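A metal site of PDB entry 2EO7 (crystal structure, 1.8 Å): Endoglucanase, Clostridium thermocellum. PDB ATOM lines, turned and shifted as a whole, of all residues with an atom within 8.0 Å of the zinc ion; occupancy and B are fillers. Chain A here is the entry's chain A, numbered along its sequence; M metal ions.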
ATOM      1  N   GLU A  33      -9.152 -31.267  23.929  1.00  0.00           N
ATOM      2  CA  GLU A  33      -8.167 -30.625  23.049  1.00  0.00           C
ATOM      3  C   GLU A  33      -8.892 -29.530  22.275  1.00  0.00           C
ATOM      4  O   GLU A  33      -9.738 -29.794  21.432  1.00  0.00           O
ATOM      5  CB  GLU A  33      -7.529 -31.668  22.123  1.00  0.00           C
ATOM      6  CG  GLU A  33      -6.892 -32.801  22.940  1.00  0.00           C
ATOM      7  CD  GLU A  33      -6.241 -33.892  22.094  1.00  0.00           C
ATOM      8  OE1 GLU A  33      -6.752 -34.200  21.001  1.00  0.00           O
ATOM      9  OE2 GLU A  33      -5.215 -34.455  22.545  1.00  0.00           O
ATOM     10  N   LEU A  34      -8.570 -28.280  22.602  1.00  0.00           N
ATOM     11  CA  LEU A  34      -9.241 -27.136  22.000  1.00  0.00           C
ATOM     12  C   LEU A  34      -8.399 -26.384  20.993  1.00  0.00           C
ATOM     13  O   LEU A  34      -7.181 -26.527  20.961  1.00  0.00           O
ATOM     14  CB  LEU A  34      -9.635 -26.132  23.083  1.00  0.00           C
ATOM     15  CG  LEU A  34     -10.586 -26.546  24.188  1.00  0.00           C
ATOM     16  CD1 LEU A  34     -10.839 -25.323  25.116  1.00  0.00           C
ATOM     17  CD2 LEU A  34     -11.885 -27.044  23.593  1.00  0.00           C
ATOM     18  N   ASP A  35      -9.088 -25.586  20.183  1.00  0.00           N
ATOM     19  CA  ASP A  35      -8.443 -24.705  19.204  1.00  0.00           C
ATOM     20  C   ASP A  35      -8.269 -23.379  19.970  1.00  0.00           C
ATOM     21  O   ASP A  35      -8.871 -22.349  19.634  1.00  0.00           O
ATOM     22  CB  ASP A  35      -9.347 -24.464  18.000  1.00  0.00           C
ATOM     23  CG  ASP A  35      -9.761 -25.767  17.319  1.00  0.00           C
ATOM     24  OD1 ASP A  35      -8.872 -26.582  17.049  1.00  0.00           O
ATOM     25  OD2 ASP A  35     -10.976 -25.948  17.056  1.00  0.00           O
ATOM     26  N   ALA A  36      -7.478 -23.441  21.028  1.00  0.00           N
ATOM     27  CA  ALA A  36      -7.221 -22.279  21.863  1.00  0.00           C
ATOM     28  C   ALA A  36      -5.969 -22.551  22.653  1.00  0.00           C
ATOM     29  O   ALA A  36      -5.589 -23.705  22.873  1.00  0.00           O
ATOM     30  CB  ALA A  36      -8.411 -22.021  22.821  1.00  0.00           C
ATOM     31  N   GLY A 365     -21.655 -22.364  22.784  1.00  0.00           N
ATOM     32  CA  GLY A 365     -20.263 -22.434  22.364  1.00  0.00           C
ATOM     33  C   GLY A 365     -19.944 -21.974  20.948  1.00  0.00           C
ATOM     34  O   GLY A 365     -18.827 -21.516  20.679  1.00  0.00           O
ATOM     35  N   ASP A 394     -15.819 -29.599  23.548  1.00  0.00           N
ATOM     36  CA  ASP A 394     -14.871 -29.839  22.458  1.00  0.00           C
ATOM     37  C   ASP A 394     -14.535 -28.658  21.558  1.00  0.00           C
ATOM     38  O   ASP A 394     -15.010 -27.535  21.753  1.00  0.00           O
ATOM     39  CB  ASP A 394     -15.328 -31.039  21.603  1.00  0.00           C
ATOM     40  CG  ASP A 394     -16.597 -30.759  20.827  1.00  0.00           C
ATOM     41  OD1 ASP A 394     -16.808 -29.602  20.412  1.00  0.00           O
ATOM     42  OD2 ASP A 394     -17.387 -31.702  20.621  1.00  0.00           O
ATOM     43  N   ALA A 395     -13.688 -28.928  20.573  1.00  0.00           N
ATOM     44  CA  ALA A 395     -13.213 -27.906  19.636  1.00  0.00           C
ATOM     45  C   ALA A 395     -14.267 -27.235  18.740  1.00  0.00           C
ATOM     46  O   ALA A 395     -13.953 -26.274  18.027  1.00  0.00           O
ATOM     47  CB  ALA A 395     -12.085 -28.482  18.776  1.00  0.00           C
ATOM     48  N   SER A 396     -15.502 -27.721  18.784  1.00  0.00           N
ATOM     49  CA  SER A 396     -16.547 -27.125  17.957  1.00  0.00           C
ATOM     50  C   SER A 396     -17.100 -25.844  18.606  1.00  0.00           C
ATOM     51  O   SER A 396     -17.880 -25.119  17.999  1.00  0.00           O
ATOM     52  CB  SER A 396     -17.707 -28.130  17.751  1.00  0.00           C
ATOM     53  OG  SER A 396     -18.424 -28.361  18.957  1.00  0.00           O
ATOM     54  N   ASN A 397     -16.684 -25.569  19.837  1.00  0.00           N
ATOM     55  CA  ASN A 397     -17.153 -24.371  20.546  1.00  0.00           C
ATOM     56  C   ASN A 397     -16.211 -23.223  20.168  1.00  0.00           C
ATOM     57  O   ASN A 397     -15.453 -22.733  21.002  1.00  0.00           O
ATOM     58  CB  ASN A 397     -17.096 -24.633  22.055  1.00  0.00           C
ATOM     59  CG  ASN A 397     -18.119 -25.661  22.491  1.00  0.00           C
ATOM     60  OD1 ASN A 397     -19.324 -25.400  22.476  1.00  0.00           O
ATOM     61  ND2 ASN A 397     -17.646 -26.840  22.885  1.00  0.00           N
ATOM     62  N   ASN A 398     -16.297 -22.787  18.905  1.00  0.00           N
ATOM     63  CA  ASN A 398     -15.408 -21.747  18.412  1.00  0.00           C
ATOM     64  C   ASN A 398     -15.460 -20.420  19.155  1.00  0.00           C
ATOM     65  O   ASN A 398     -14.428 -19.746  19.311  1.00  0.00           O
ATOM     66  CB  ASN A 398     -15.631 -21.515  16.906  1.00  0.00           C
ATOM     67  CG  ASN A 398     -17.065 -21.152  16.557  1.00  0.00           C
ATOM     68  OD1 ASN A 398     -17.999 -21.869  16.903  1.00  0.00           O
ATOM     69  ND2 ASN A 398     -17.237 -20.038  15.845  1.00  0.00           N
ATOM     70  N   TYR A 399     -16.647 -20.029  19.600  1.00  0.00           N
ATOM     71  CA  TYR A 399     -16.712 -18.761  20.332  1.00  0.00           C
ATOM     72  C   TYR A 399     -16.188 -18.926  21.752  1.00  0.00           C
ATOM     73  O   TYR A 399     -15.575 -18.009  22.285  1.00  0.00           O
ATOM     74  CB  TYR A 399     -18.137 -18.198  20.308  1.00  0.00           C
ATOM     75  CG  TYR A 399     -18.366 -17.320  19.091  1.00  0.00           C
ATOM     76  CD1 TYR A 399     -17.816 -16.033  19.018  1.00  0.00           C
ATOM     77  CD2 TYR A 399     -19.096 -17.778  17.992  1.00  0.00           C
ATOM     78  CE1 TYR A 399     -17.996 -15.232  17.884  1.00  0.00           C
ATOM     79  CE2 TYR A 399     -19.277 -16.986  16.855  1.00  0.00           C
ATOM     80  CZ  TYR A 399     -18.727 -15.708  16.803  1.00  0.00           C
ATOM     81  OH  TYR A 399     -18.916 -14.916  15.694  1.00  0.00           O
ATOM     82  N   THR A 400     -16.407 -20.078  22.363  1.00  0.00           N
ATOM     83  CA  THR A 400     -15.844 -20.322  23.695  1.00  0.00           C
ATOM     84  C   THR A 400     -14.315 -20.205  23.559  1.00  0.00           C
ATOM     85  O   THR A 400     -13.638 -19.600  24.385  1.00  0.00           O
ATOM     86  CB  THR A 400     -16.163 -21.746  24.209  1.00  0.00           C
ATOM     87  OG1 THR A 400     -17.580 -21.963  24.179  1.00  0.00           O
ATOM     88  CG2 THR A 400     -15.663 -21.913  25.667  1.00  0.00           C
ATOM     89  N   GLU A 401     -13.778 -20.812  22.500  1.00  0.00           N
ATOM     90  CA  GLU A 401     -12.338 -20.752  22.271  1.00  0.00           C
ATOM     91  C   GLU A 401     -11.860 -19.328  22.059  1.00  0.00           C
ATOM     92  O   GLU A 401     -10.769 -18.972  22.521  1.00  0.00           O
ATOM     93  CB  GLU A 401     -11.981 -21.634  21.071  1.00  0.00           C
ATOM     94  CG  GLU A 401     -12.296 -23.122  21.347  1.00  0.00           C
ATOM     95  CD  GLU A 401     -12.182 -23.967  20.100  1.00  0.00           C
ATOM     96  OE1 GLU A 401     -12.522 -23.446  19.012  1.00  0.00           O
ATOM     97  OE2 GLU A 401     -11.780 -25.143  20.209  1.00  0.00           O
ATOM     98  N   ALA A 402     -12.658 -18.498  21.390  1.00  0.00           N
ATOM     99  CA  ALA A 402     -12.271 -17.098  21.217  1.00  0.00           C
ATOM    100  C   ALA A 402     -12.233 -16.416  22.582  1.00  0.00           C
ATOM    101  O   ALA A 402     -11.341 -15.604  22.877  1.00  0.00           O
ATOM    102  CB  ALA A 402     -13.252 -16.372  20.295  1.00  0.00           C
ATOM    103  N   SER A 484     -15.467 -15.482  14.938  1.00  0.00           N
ATOM    104  CA  SER A 484     -14.936 -15.849  16.237  1.00  0.00           C
ATOM    105  C   SER A 484     -13.410 -15.660  16.190  1.00  0.00           C
ATOM    106  O   SER A 484     -12.741 -15.772  17.204  1.00  0.00           O
ATOM    107  CB  SER A 484     -15.291 -17.299  16.593  1.00  0.00           C
ATOM    108  OG  SER A 484     -14.964 -18.209  15.546  1.00  0.00           O
HETATM  109 ZN    ZN M   1     -12.547 -24.935  17.650  1.00  0.00          ZN
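The zinc ion is bound by the side-chain carboxylate (OD2) of Asp 35, the backbone carbonyl oxygen (O) of Ala 395 and the side-chain carboxylate (OE1) of Glu 401. Slightly farther from the zinc ion lies the side-chain carboxylate (OE2) of Glu 401 (2.7 Å).
Within 4 Å of the zinc ion: Asp 35, Ala 395 and Glu 401.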
